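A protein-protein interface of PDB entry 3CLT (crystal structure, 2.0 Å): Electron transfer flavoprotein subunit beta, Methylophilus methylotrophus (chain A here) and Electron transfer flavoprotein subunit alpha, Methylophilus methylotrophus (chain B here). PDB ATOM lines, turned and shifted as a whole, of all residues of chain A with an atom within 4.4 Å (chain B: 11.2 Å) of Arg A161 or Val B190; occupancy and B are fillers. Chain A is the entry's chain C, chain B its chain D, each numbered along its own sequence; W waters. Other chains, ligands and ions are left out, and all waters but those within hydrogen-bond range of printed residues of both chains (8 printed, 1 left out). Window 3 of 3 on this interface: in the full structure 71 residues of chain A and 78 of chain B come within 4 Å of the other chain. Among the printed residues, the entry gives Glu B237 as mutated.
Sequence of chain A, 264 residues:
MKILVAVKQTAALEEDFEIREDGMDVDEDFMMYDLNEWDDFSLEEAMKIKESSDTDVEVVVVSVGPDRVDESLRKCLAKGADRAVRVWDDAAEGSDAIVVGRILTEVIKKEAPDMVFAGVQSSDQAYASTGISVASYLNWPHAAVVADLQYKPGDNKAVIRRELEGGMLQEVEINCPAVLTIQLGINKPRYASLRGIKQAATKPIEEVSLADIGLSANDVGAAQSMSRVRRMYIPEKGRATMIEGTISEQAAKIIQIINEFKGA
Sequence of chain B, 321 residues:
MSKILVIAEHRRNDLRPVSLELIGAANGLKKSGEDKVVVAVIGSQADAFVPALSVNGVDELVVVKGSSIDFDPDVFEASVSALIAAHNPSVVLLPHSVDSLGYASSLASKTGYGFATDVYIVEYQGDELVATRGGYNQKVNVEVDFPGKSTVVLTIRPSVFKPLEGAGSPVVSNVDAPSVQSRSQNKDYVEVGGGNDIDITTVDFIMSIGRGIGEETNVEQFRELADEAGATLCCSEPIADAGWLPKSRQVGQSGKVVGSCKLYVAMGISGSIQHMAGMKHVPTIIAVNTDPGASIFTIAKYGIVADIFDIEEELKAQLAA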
ATOM      1  N   VAL A 145      27.838  17.011 -16.248  1.00  0.00           N
ATOM      2  CA  VAL A 145      28.378  16.309 -15.072  1.00  0.00           C
ATOM      3  C   VAL A 145      28.951  14.946 -15.467  1.00  0.00           C
ATOM      4  O   VAL A 145      28.594  13.906 -14.906  1.00  0.00           O
ATOM      5  CB  VAL A 145      27.377  16.219 -13.891  1.00  0.00           C
ATOM      6  CG1 VAL A 145      28.107  15.947 -12.590  1.00  0.00           C
ATOM      7  CG2 VAL A 145      26.553  17.518 -13.769  1.00  0.00           C
ATOM      8  N   VAL A 146      29.864  14.980 -16.427  1.00  0.00           N
ATOM      9  CA  VAL A 146      30.474  13.771 -16.975  1.00  0.00           C
ATOM     10  C   VAL A 146      31.678  13.337 -16.121  1.00  0.00           C
ATOM     11  O   VAL A 146      32.674  14.073 -15.978  1.00  0.00           O
ATOM     12  CB  VAL A 146      30.873  13.985 -18.456  1.00  0.00           C
ATOM     13  CG1 VAL A 146      31.700  12.813 -18.984  1.00  0.00           C
ATOM     14  CG2 VAL A 146      29.634  14.222 -19.302  1.00  0.00           C
ATOM     15  N   ALA A 147      31.570  12.140 -15.563  1.00  0.00           N
ATOM     16  CA  ALA A 147      32.583  11.564 -14.687  1.00  0.00           C
ATOM     17  C   ALA A 147      33.372  10.448 -15.349  1.00  0.00           C
ATOM     18  O   ALA A 147      34.318   9.939 -14.760  1.00  0.00           O
ATOM     19  CB  ALA A 147      31.929  11.032 -13.423  1.00  0.00           C
ATOM     20  N   ASP A 148      32.962  10.050 -16.552  1.00  0.00           N
ATOM     21  CA  ASP A 148      33.672   9.050 -17.328  1.00  0.00           C
ATOM     22  C   ASP A 148      33.342   9.270 -18.799  1.00  0.00           C
ATOM     23  O   ASP A 148      32.197   9.599 -19.144  1.00  0.00           O
ATOM     24  CB  ASP A 148      33.265   7.624 -16.906  1.00  0.00           C
ATOM     25  CG  ASP A 148      34.162   6.558 -17.510  1.00  0.00           C
ATOM     26  OD1 ASP A 148      33.741   5.867 -18.464  1.00  0.00           O
ATOM     27  OD2 ASP A 148      35.301   6.422 -17.042  1.00  0.00           O
ATOM     28  N   ILE A 160      29.284   8.011 -22.039  1.00  0.00           N
ATOM     29  CA  ILE A 160      29.656   8.784 -20.859  1.00  0.00           C
ATOM     30  C   ILE A 160      28.943   8.227 -19.651  1.00  0.00           C
ATOM     31  O   ILE A 160      27.947   7.520 -19.788  1.00  0.00           O
ATOM     32  CB  ILE A 160      29.370  10.333 -20.997  1.00  0.00           C
ATOM     33  CG1 ILE A 160      27.893  10.655 -21.277  1.00  0.00           C
ATOM     34  CG2 ILE A 160      30.247  10.945 -22.097  1.00  0.00           C
ATOM     35  CD1 ILE A 160      27.086  11.112 -20.068  1.00  0.00           C
ATOM     36  N   ARG A 161      29.467   8.558 -18.475  1.00  0.00           N
ATOM     37  CA  ARG A 161      28.737   8.364 -17.226  1.00  0.00           C
ATOM     38  C   ARG A 161      28.520   9.707 -16.586  1.00  0.00           C
ATOM     39  O   ARG A 161      29.479  10.455 -16.324  1.00  0.00           O
ATOM     40  CB  ARG A 161      29.477   7.415 -16.285  1.00  0.00           C
ATOM     41  CG  ARG A 161      29.455   5.990 -16.802  1.00  0.00           C
ATOM     42  CD  ARG A 161      30.331   5.049 -16.017  1.00  0.00           C
ATOM     43  NE  ARG A 161      30.091   3.683 -16.475  1.00  0.00           N
ATOM     44  CZ  ARG A 161      30.384   2.579 -15.793  1.00  0.00           C
ATOM     45  NH1 ARG A 161      30.941   2.645 -14.593  1.00  0.00           N
ATOM     46  NH2 ARG A 161      30.096   1.402 -16.319  1.00  0.00           N
ATOM     47  N   ARG A 162      27.264  10.052 -16.345  1.00  0.00           N
ATOM     48  CA  ARG A 162      27.026  11.259 -15.577  1.00  0.00           C
ATOM     49  C   ARG A 162      26.864  10.932 -14.090  1.00  0.00           C
ATOM     50  O   ARG A 162      26.341   9.891 -13.715  1.00  0.00           O
ATOM     51  CB  ARG A 162      25.925  12.145 -16.173  1.00  0.00           C
ATOM     52  CG  ARG A 162      24.637  11.523 -16.379  1.00  0.00           C
ATOM     53  CD  ARG A 162      23.643  12.467 -17.037  1.00  0.00           C
ATOM     54  NE  ARG A 162      22.328  11.896 -16.796  1.00  0.00           N
ATOM     55  CZ  ARG A 162      21.347  12.438 -16.072  1.00  0.00           C
ATOM     56  NH1 ARG A 162      21.443  13.654 -15.559  1.00  0.00           N
ATOM     57  NH2 ARG A 162      20.227  11.756 -15.910  1.00  0.00           N
ATOM     58  N   GLU A 163      27.415  11.798 -13.251  1.00  0.00           N
ATOM     59  CA  GLU A 163      27.458  11.569 -11.820  1.00  0.00           C
ATOM     60  C   GLU A 163      26.219  12.147 -11.161  1.00  0.00           C
ATOM     61  O   GLU A 163      26.059  13.367 -11.082  1.00  0.00           O
ATOM     62  CB  GLU A 163      28.715  12.213 -11.229  1.00  0.00           C
ATOM     63  CG  GLU A 163      28.966  11.847  -9.783  1.00  0.00           C
ATOM     64  CD  GLU A 163      30.303  12.374  -9.293  1.00  0.00           C
ATOM     65  OE1 GLU A 163      30.344  13.495  -8.754  1.00  0.00           O
ATOM     66  OE2 GLU A 163      31.310  11.682  -9.495  1.00  0.00           O
ATOM     67  N   MET A 168      25.227   7.290  -7.296  1.00  0.00           N
ATOM     68  CA  MET A 168      25.030   6.529  -8.519  1.00  0.00           C
ATOM     69  C   MET A 168      25.386   7.335  -9.758  1.00  0.00           C
ATOM     70  O   MET A 168      25.464   8.562  -9.720  1.00  0.00           O
ATOM     71  CB  MET A 168      23.604   5.981  -8.600  1.00  0.00           C
ATOM     72  CG  MET A 168      22.523   7.002  -8.809  1.00  0.00           C
ATOM     73  SD  MET A 168      20.900   6.268  -8.482  1.00  0.00           S
ATOM     74  CE  MET A 168      21.002   6.121  -6.707  1.00  0.00           C
ATOM     75  N   LEU A 169      25.630   6.604 -10.840  1.00  0.00           N
ATOM     76  CA  LEU A 169      25.931   7.163 -12.153  1.00  0.00           C
ATOM     77  C   LEU A 169      24.899   6.691 -13.164  1.00  0.00           C
ATOM     78  O   LEU A 169      24.180   5.724 -12.927  1.00  0.00           O
ATOM     79  CB  LEU A 169      27.306   6.679 -12.637  1.00  0.00           C
ATOM     80  CG  LEU A 169      28.457   6.736 -11.630  1.00  0.00           C
ATOM     81  CD1 LEU A 169      29.636   5.942 -12.142  1.00  0.00           C
ATOM     82  CD2 LEU A 169      28.845   8.184 -11.382  1.00  0.00           C
ATOM     83  N   GLN A 170      24.845   7.374 -14.299  1.00  0.00           N
ATOM     84  CA  GLN A 170      24.080   6.890 -15.450  1.00  0.00           C
ATOM     85  C   GLN A 170      24.954   6.888 -16.695  1.00  0.00           C
ATOM     86  O   GLN A 170      25.509   7.912 -17.085  1.00  0.00           O
ATOM     87  CB  GLN A 170      22.835   7.739 -15.690  1.00  0.00           C
ATOM     88  CG  GLN A 170      21.839   7.119 -16.672  1.00  0.00           C
ATOM     89  CD  GLN A 170      20.744   8.091 -17.050  1.00  0.00           C
ATOM     90  OE1 GLN A 170      20.998   9.278 -17.207  1.00  0.00           O
ATOM     91  NE2 GLN A 170      19.528   7.599 -17.188  1.00  0.00           N
ATOM     92  N   GLU A 171      25.076   5.717 -17.303  1.00  0.00           N
ATOM     93  CA  GLU A 171      25.694   5.578 -18.596  1.00  0.00           C
ATOM     94  C   GLU A 171      24.749   6.129 -19.672  1.00  0.00           C
ATOM     95  O   GLU A 171      23.533   5.857 -19.659  1.00  0.00           O
ATOM     96  CB  GLU A 171      26.013   4.105 -18.837  1.00  0.00           C
ATOM     97  CG  GLU A 171      27.077   3.860 -19.842  1.00  0.00           C
ATOM     98  CD  GLU A 171      27.536   2.418 -19.824  1.00  0.00           C
ATOM     99  OE1 GLU A 171      27.208   1.680 -20.783  1.00  0.00           O
ATOM    100  OE2 GLU A 171      28.184   2.019 -18.824  1.00  0.00           O
ATOM    101  N   ARG B  11      13.337   9.551 -10.666  1.00  0.00           N
ATOM    102  CA  ARG B  11      14.419   8.697 -11.144  1.00  0.00           C
ATOM    103  C   ARG B  11      14.188   7.308 -10.577  1.00  0.00           C
ATOM    104  O   ARG B  11      13.819   7.183  -9.415  1.00  0.00           O
ATOM    105  CB  ARG B  11      15.772   9.267 -10.676  1.00  0.00           C
ATOM    106  CG  ARG B  11      16.968   8.310 -10.756  1.00  0.00           C
ATOM    107  CD  ARG B  11      18.255   9.014 -10.378  1.00  0.00           C
ATOM    108  NE  ARG B  11      18.495  10.177 -11.229  1.00  0.00           N
ATOM    109  CZ  ARG B  11      18.913  11.373 -10.817  1.00  0.00           C
ATOM    110  NH1 ARG B  11      19.150  11.628  -9.532  1.00  0.00           N
ATOM    111  NH2 ARG B  11      19.079  12.330 -11.711  1.00  0.00           N
ATOM    112  N   ARG B  12      14.386   6.278 -11.395  1.00  0.00           N
ATOM    113  CA  ARG B  12      14.243   4.875 -10.946  1.00  0.00           C
ATOM    114  C   ARG B  12      12.914   4.601 -10.249  1.00  0.00           C
ATOM    115  O   ARG B  12      12.891   3.957  -9.196  1.00  0.00           O
ATOM    116  CB  ARG B  12      15.361   4.486  -9.966  1.00  0.00           C
ATOM    117  CG  ARG B  12      16.761   4.489 -10.522  1.00  0.00           C
ATOM    118  CD  ARG B  12      17.705   3.721  -9.576  1.00  0.00           C
ATOM    119  NE  ARG B  12      17.716   4.259  -8.215  1.00  0.00           N
ATOM    120  CZ  ARG B  12      18.501   3.816  -7.234  1.00  0.00           C
ATOM    121  NH1 ARG B  12      19.357   2.818  -7.443  1.00  0.00           N
ATOM    122  NH2 ARG B  12      18.433   4.376  -6.034  1.00  0.00           N
ATOM    123  N   ASP B  70      13.433   8.116 -17.882  1.00  0.00           N
ATOM    124  CA  ASP B  70      13.972   9.157 -17.009  1.00  0.00           C
ATOM    125  C   ASP B  70      14.589  10.309 -17.831  1.00  0.00           C
ATOM    126  O   ASP B  70      14.407  10.388 -19.038  1.00  0.00           O
ATOM    127  CB  ASP B  70      14.991   8.549 -16.031  1.00  0.00           C
ATOM    128  CG  ASP B  70      14.351   7.581 -15.015  1.00  0.00           C
ATOM    129  OD1 ASP B  70      13.109   7.586 -14.858  1.00  0.00           O
ATOM    130  OD2 ASP B  70      15.095   6.814 -14.363  1.00  0.00           O
ATOM    131  N   PHE B  71      15.305  11.203 -17.166  1.00  0.00           N
ATOM    132  CA  PHE B  71      15.804  12.402 -17.787  1.00  0.00           C
ATOM    133  C   PHE B  71      16.595  12.211 -19.076  1.00  0.00           C
ATOM    134  O   PHE B  71      17.486  11.373 -19.163  1.00  0.00           O
ATOM    135  CB  PHE B  71      16.686  13.161 -16.821  1.00  0.00           C
ATOM    136  CG  PHE B  71      17.299  14.380 -17.425  1.00  0.00           C
ATOM    137  CD1 PHE B  71      16.532  15.517 -17.632  1.00  0.00           C
ATOM    138  CD2 PHE B  71      18.633  14.392 -17.793  1.00  0.00           C
ATOM    139  CE1 PHE B  71      17.080  16.637 -18.206  1.00  0.00           C
ATOM    140  CE2 PHE B  71      19.187  15.511 -18.358  1.00  0.00           C
ATOM    141  CZ  PHE B  71      18.403  16.635 -18.572  1.00  0.00           C
ATOM    142  N   VAL B  98      21.359  17.626 -10.882  1.00  0.00           N
ATOM    143  CA  VAL B  98      22.182  17.141 -11.991  1.00  0.00           C
ATOM    144  C   VAL B  98      21.377  17.075 -13.307  1.00  0.00           C
ATOM    145  O   VAL B  98      21.875  17.455 -14.371  1.00  0.00           O
ATOM    146  CB  VAL B  98      22.844  15.786 -11.637  1.00  0.00           C
ATOM    147  CG1 VAL B  98      23.574  15.196 -12.838  1.00  0.00           C
ATOM    148  CG2 VAL B  98      23.815  15.974 -10.462  1.00  0.00           C
ATOM    149  N   ASP B  99      20.133  16.608 -13.232  1.00  0.00           N
ATOM    150  CA  ASP B  99      19.245  16.593 -14.401  1.00  0.00           C
ATOM    151  C   ASP B  99      19.080  18.003 -14.994  1.00  0.00           C
ATOM    152  O   ASP B  99      19.325  18.218 -16.179  1.00  0.00           O
ATOM    153  CB  ASP B  99      17.872  16.028 -14.035  1.00  0.00           C
ATOM    154  CG  ASP B  99      17.851  14.503 -13.908  1.00  0.00           C
ATOM    155  OD1 ASP B  99      18.878  13.831 -14.139  1.00  0.00           O
ATOM    156  OD2 ASP B  99      16.776  13.964 -13.573  1.00  0.00           O
ATOM    157  N   SER B 184      20.971  11.599 -27.725  1.00  0.00           N
ATOM    158  CA  SER B 184      21.591  10.643 -26.819  1.00  0.00           C
ATOM    159  C   SER B 184      20.576   9.559 -26.414  1.00  0.00           C
ATOM    160  O   SER B 184      19.364   9.695 -26.649  1.00  0.00           O
ATOM    161  CB  SER B 184      22.251  11.337 -25.595  1.00  0.00           C
ATOM    162  OG  SER B 184      21.342  12.040 -24.750  1.00  0.00           O
ATOM    163  N   GLN B 185      21.098   8.464 -25.874  1.00  0.00           N
ATOM    164  CA  GLN B 185      20.291   7.363 -25.372  1.00  0.00           C
ATOM    165  C   GLN B 185      20.827   6.929 -24.006  1.00  0.00           C
ATOM    166  O   GLN B 185      22.017   6.654 -23.851  1.00  0.00           O
ATOM    167  CB  GLN B 185      20.330   6.198 -26.369  1.00  0.00           C
ATOM    168  CG  GLN B 185      19.698   4.907 -25.873  1.00  0.00           C
ATOM    169  CD  GLN B 185      18.183   4.990 -25.711  1.00  0.00           C
ATOM    170  OE1 GLN B 185      17.480   5.580 -26.558  1.00  0.00           O
ATOM    171  NE2 GLN B 185      17.664   4.381 -24.622  1.00  0.00           N
ATOM    172  N   ASN B 186      19.930   6.867 -23.029  1.00  0.00           N
ATOM    173  CA  ASN B 186      20.273   6.461 -21.678  1.00  0.00           C
ATOM    174  C   ASN B 186      20.487   4.954 -21.630  1.00  0.00           C
ATOM    175  O   ASN B 186      19.760   4.199 -22.265  1.00  0.00           O
ATOM    176  CB  ASN B 186      19.153   6.804 -20.709  1.00  0.00           C
ATOM    177  CG  ASN B 186      18.967   8.288 -20.520  1.00  0.00           C
ATOM    178  OD1 ASN B 186      19.888   9.089 -20.747  1.00  0.00           O
ATOM    179  ND2 ASN B 186      17.766   8.673 -20.077  1.00  0.00           N
ATOM    180  N   LYS B 187      21.497   4.534 -20.881  1.00  0.00           N
ATOM    181  CA  LYS B 187      21.818   3.117 -20.736  1.00  0.00           C
ATOM    182  C   LYS B 187      21.741   2.794 -19.239  1.00  0.00           C
ATOM    183  O   LYS B 187      20.902   3.372 -18.542  1.00  0.00           O
ATOM    184  CB  LYS B 187      23.170   2.827 -21.385  1.00  0.00           C
ATOM    185  CG  LYS B 187      23.254   3.234 -22.875  1.00  0.00           C
ATOM    186  CD  LYS B 187      22.371   2.347 -23.769  1.00  0.00           C
ATOM    187  CE  LYS B 187      22.474   2.715 -25.249  1.00  0.00           C
ATOM    188  NZ  LYS B 187      21.606   1.837 -26.101  1.00  0.00           N
ATOM    189  N   ASP B 188      22.584   1.900 -18.727  1.00  0.00           N
ATOM    190  CA  ASP B 188      22.442   1.438 -17.340  1.00  0.00           C
ATOM    191  C   ASP B 188      22.665   2.549 -16.311  1.00  0.00           C
ATOM    192  O   ASP B 188      23.496   3.438 -16.505  1.00  0.00           O
ATOM    193  CB  ASP B 188      23.438   0.303 -17.035  1.00  0.00           C
ATOM    194  CG  ASP B 188      23.144  -0.975 -17.792  1.00  0.00           C
ATOM    195  OD1 ASP B 188      21.983  -1.227 -18.135  1.00  0.00           O
ATOM    196  OD2 ASP B 188      24.089  -1.756 -18.005  1.00  0.00           O
ATOM    197  N   TYR B 189      21.931   2.476 -15.203  1.00  0.00           N
ATOM    198  CA  TYR B 189      22.397   3.094 -13.961  1.00  0.00           C
ATOM    199  C   TYR B 189      23.505   2.209 -13.396  1.00  0.00           C
ATOM    200  O   TYR B 189      23.509   0.977 -13.597  1.00  0.00           O
ATOM    201  CB  TYR B 189      21.257   3.263 -12.945  1.00  0.00           C
ATOM    202  CG  TYR B 189      20.246   4.312 -13.341  1.00  0.00           C
ATOM    203  CD1 TYR B 189      18.956   3.963 -13.735  1.00  0.00           C
ATOM    204  CD2 TYR B 189      20.590   5.656 -13.334  1.00  0.00           C
ATOM    205  CE1 TYR B 189      18.020   4.941 -14.103  1.00  0.00           C
ATOM    206  CE2 TYR B 189      19.678   6.637 -13.693  1.00  0.00           C
ATOM    207  CZ  TYR B 189      18.391   6.284 -14.066  1.00  0.00           C
ATOM    208  OH  TYR B 189      17.508   7.268 -14.445  1.00  0.00           O
ATOM    209  N   VAL B 190      24.450   2.838 -12.708  1.00  0.00           N
ATOM    210  CA  VAL B 190      25.633   2.163 -12.187  1.00  0.00           C
ATOM    211  C   VAL B 190      25.974   2.670 -10.791  1.00  0.00           C
ATOM    212  O   VAL B 190      25.858   3.865 -10.513  1.00  0.00           O
ATOM    213  CB  VAL B 190      26.886   2.422 -13.086  1.00  0.00           C
ATOM    214  CG1 VAL B 190      28.089   1.643 -12.577  1.00  0.00           C
ATOM    215  CG2 VAL B 190      26.618   2.046 -14.545  1.00  0.00           C
ATOM    216  N   GLU B 191      26.386   1.750  -9.921  1.00  0.00           N
ATOM    217  CA  GLU B 191      27.115   2.090  -8.702  1.00  0.00           C
ATOM    218  C   GLU B 191      28.529   1.510  -8.792  1.00  0.00           C
ATOM    219  O   GLU B 191      28.704   0.295  -8.964  1.00  0.00           O
ATOM    220  CB  GLU B 191      26.341   1.607  -7.471  1.00  0.00           C
ATOM    221  CG  GLU B 191      25.068   2.439  -7.329  1.00  0.00           C
ATOM    222  CD  GLU B 191      24.257   2.206  -6.074  1.00  0.00           C
ATOM    223  OE1 GLU B 191      24.818   1.765  -5.044  1.00  0.00           O
ATOM    224  OE2 GLU B 191      23.043   2.520  -6.127  1.00  0.00           O
ATOM    225  N   VAL B 192      29.541   2.376  -8.718  1.00  0.00           N
ATOM    226  CA  VAL B 192      30.935   1.938  -8.948  1.00  0.00           C
ATOM    227  C   VAL B 192      31.493   1.107  -7.796  1.00  0.00           C
ATOM    228  O   VAL B 192      31.025   1.198  -6.662  1.00  0.00           O
ATOM    229  CB  VAL B 192      31.929   3.116  -9.265  1.00  0.00           C
ATOM    230  CG1 VAL B 192      31.468   3.896 -10.479  1.00  0.00           C
ATOM    231  CG2 VAL B 192      32.121   4.040  -8.071  1.00  0.00           C
ATOM    232  N   GLY B 193      32.506   0.303  -8.113  1.00  0.00           N
ATOM    233  CA  GLY B 193      33.153  -0.583  -7.149  1.00  0.00           C
ATOM    234  C   GLY B 193      33.766   0.187  -5.998  1.00  0.00           C
ATOM    235  O   GLY B 193      33.570   1.397  -5.851  1.00  0.00           O
ATOM    236  N   GLY B 194      34.525  -0.524  -5.185  1.00  0.00           N
ATOM    237  CA  GLY B 194      35.090   0.036  -3.973  1.00  0.00           C
ATOM    238  C   GLY B 194      34.353  -0.539  -2.791  1.00  0.00           C
ATOM    239  O   GLY B 194      33.170  -0.912  -2.896  1.00  0.00           O
ATOM    240  N   ASN B 196      32.450  -1.386   0.691  1.00  0.00           N
ATOM    241  CA  ASN B 196      31.136  -0.979   1.153  1.00  0.00           C
ATOM    242  C   ASN B 196      30.793  -1.760   2.423  1.00  0.00           C
ATOM    243  O   ASN B 196      29.776  -2.456   2.490  1.00  0.00           O
ATOM    244  CB  ASN B 196      30.107  -1.235   0.047  1.00  0.00           C
ATOM    245  CG  ASN B 196      28.887  -0.334   0.147  1.00  0.00           C
ATOM    246  OD1 ASN B 196      28.804   0.536   1.022  1.00  0.00           O
ATOM    247  ND2 ASN B 196      27.936  -0.520  -0.773  1.00  0.00           N
ATOM    248  N   GLU B 237      34.602  14.875  -1.215  1.00  0.00           N
ATOM    249  CA  GLU B 237      34.802  14.315  -2.550  1.00  0.00           C
ATOM    250  C   GLU B 237      36.267  14.127  -2.967  1.00  0.00           C
ATOM    251  O   GLU B 237      36.595  13.088  -3.517  1.00  0.00           O
ATOM    252  CB  GLU B 237      34.056  15.133  -3.620  1.00  0.00           C
ATOM    253  CG  GLU B 237      34.336  14.616  -5.005  1.00  0.00           C
ATOM    254  CD  GLU B 237      33.518  15.246  -6.107  1.00  0.00           C
ATOM    255  OE1 GLU B 237      32.522  15.913  -5.819  1.00  0.00           O
ATOM    256  OE2 GLU B 237      33.875  15.042  -7.281  1.00  0.00           O
ATOM    257  N   LYS B 247      34.208   5.253  -2.155  1.00  0.00           N
ATOM    258  CA  LYS B 247      33.130   6.187  -2.494  1.00  0.00           C
ATOM    259  C   LYS B 247      31.982   6.071  -1.497  1.00  0.00           C
ATOM    260  O   LYS B 247      31.282   7.042  -1.237  1.00  0.00           O
ATOM    261  CB  LYS B 247      32.585   5.921  -3.905  1.00  0.00           C
ATOM    262  CG  LYS B 247      33.555   6.149  -5.044  1.00  0.00           C
ATOM    263  CD  LYS B 247      34.130   7.552  -5.063  1.00  0.00           C
ATOM    264  CE  LYS B 247      33.264   8.565  -5.778  1.00  0.00           C
ATOM    265  NZ  LYS B 247      33.924   9.925  -5.721  1.00  0.00           N
ATOM    266  N   SER B 254      26.826  14.142  -4.463  1.00  0.00           N
ATOM    267  CA  SER B 254      27.232  12.996  -5.262  1.00  0.00           C
ATOM    268  C   SER B 254      27.440  11.730  -4.409  1.00  0.00           C
ATOM    269  O   SER B 254      27.390  10.609  -4.919  1.00  0.00           O
ATOM    270  CB  SER B 254      28.523  13.323  -6.026  1.00  0.00           C
ATOM    271  OG  SER B 254      28.239  14.030  -7.222  1.00  0.00           O
ATOM    272  N   GLY B 255      27.700  11.926  -3.121  1.00  0.00           N
ATOM    273  CA  GLY B 255      27.847  10.825  -2.177  1.00  0.00           C
ATOM    274  C   GLY B 255      26.549  10.608  -1.429  1.00  0.00           C
ATOM    275  O   GLY B 255      25.468  10.658  -2.023  1.00  0.00           O
ATOM    276  N   LYS B 256      26.660  10.406  -0.120  1.00  0.00           N
ATOM    277  CA  LYS B 256      25.510  10.053   0.715  1.00  0.00           C
ATOM    278  C   LYS B 256      25.115  11.170   1.669  1.00  0.00           C
ATOM    279  O   LYS B 256      25.948  12.011   2.057  1.00  0.00           O
ATOM    280  CB  LYS B 256      25.825   8.807   1.535  1.00  0.00           C
ATOM    281  CG  LYS B 256      26.262   7.600   0.715  1.00  0.00           C
ATOM    282  CD  LYS B 256      25.080   6.927   0.045  1.00  0.00           C
ATOM    283  CE  LYS B 256      25.501   5.677  -0.708  1.00  0.00           C
ATOM    284  NZ  LYS B 256      24.568   5.402  -1.839  1.00  0.00           N
HETATM  285  O   HOH W   1      25.928  14.945  -8.200  1.00  0.00           O
HETATM  286  O   HOH W   2      23.192  15.950 -16.325  1.00  0.00           O
HETATM  287  O   HOH W   3      18.074   9.993 -14.180  1.00  0.00           O
HETATM  288  O   HOH W   4      19.931   9.650  -7.372  1.00  0.00           O
HETATM  289  O   HOH W   5      24.885   0.411 -19.975  1.00  0.00           O
HETATM  290  O   HOH W   6      19.299   4.692 -16.921  1.00  0.00           O
HETATM  291  O   HOH W   7      27.286   9.761  -7.523  1.00  0.00           O
HETATM  292  O   HOH W   8      32.208  12.369  -6.591  1.00  0.00           O
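The side-chain hydroxyl (OH) of Tyr B189 is in hydrogen-bond range of the side-chain amide nitrogen (NE2) of Gln A170. The side-chain carboxylate (OE1) of Glu A163 is in hydrogen-bond range of the side-chain hydroxyl (OG) of Ser B254 (2.7 Å). The side-chain sulfur (SD) of Met A168 sits close to the guanidinium group (NE) of Arg B12, 3.8 Å away. O of Val B190 lies within hydrogen-bond range of N of Leu A169, 2.8 Å away. NH1 of Arg A162 is in salt-bridge range of OD1 of Asp B99, 2.9 Å away. N of Glu A171 sits at hydrogen-bond distance from O of Asp B188 (2.9 Å). N of Lys B187 sits at hydrogen-bond distance from O of Glu A171 (2.7 Å).
The guanidinium group of Arg A161 lies within salt-bridge range of the side-chain carboxylate of Glu A171. The guanidinium group (NH1) of Arg B12 lies within salt-bridge range of the side-chain carboxylate (OE2) of Glu B191, 3.9 Å away.
CG2 of Val A145 touches CG1 of Val B98, at 3.9 Å. Arg A161 touches Val B190 (NH1 to CG1, 3.6 Å). NH1 of Arg A162 touches CG1 of Val B98, at 3.8 Å. Val B98 touches Glu A163 (CG2 to O, 3.5 Å). CA of Met A168 touches O of Val B190 (3.4 Å). Leu A169 touches Tyr B189 (O to CA, 3.3 Å). O of Glu A171 touches C of Asn B186, at 3.7 Å.
Ala A147 touches none of the printed residues of chain B. No residue of chain B comes within 4 Å of Asp A148. No residue of chain B comes within 4 Å of Ile A160. Arg A161 touches just one residue of chain B: Val B190. Of the printed residues of chain B, Arg A162 touches Phe B71 (3.6 Å), Val B98 (3.8 Å) and Asp B99 (2.9 Å). Of the printed residues of chain B, Met A168 touches Arg B12 and Val B190. Of chain B, only Tyr B189, Val B190 and Val B192 come within 4 Å of Leu A169. Of the printed residues of chain A, Asn B186 touches Gln A170 and Glu A171. Val B190 touches just these residues of chain A: Arg A161, Met A168 and Leu A169. The nearest residue of chain B that does not touch Arg A161 is Val B192 (4.3 Å). The nearest printed residue of chain A that does not touch Val B190 is Glu A171 (4.6 Å). The nearest printed residue of chain B that does not touch Glu A163 is Glu B237 (4.1 Å).
Printed residues of chain A that touch a printed residue of chain B: Val A145, Arg A161, Arg A162, Glu A163, Met A168, Leu A169, Gln A170 and Glu A171. Hydrophobic or aromatic side chains of chain A that line the printed part of chain B: Val A145, Met A168 and Leu A169. Of the 23 printed residues of chain B, 11 touch a printed residue of chain A. Hydrophobic or aromatic side chains of chain B within 4 Å of the printed part of chain A: Phe B71, Val B98, Tyr B189, Val B190 and Val B192. Among the printed residues, 18 pairs touch across the chains. Among the printed residues, Asp or Glu carboxylates within 4 Å of a Lys or Arg side-chain nitrogen of the other chain: Arg A162 with Asp B99 (2.9 Å).
Water W1 lies within hydrogen-bond range of OG of Ser B254 (2.7 Å) and O of Glu A163 (3.3 Å). Water W8 lies within hydrogen-bond range of OE1 of Glu A163 (3.1 Å), NZ of Lys B247 (3.1 Å) and OE2 of Glu B237 (3.2 Å).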
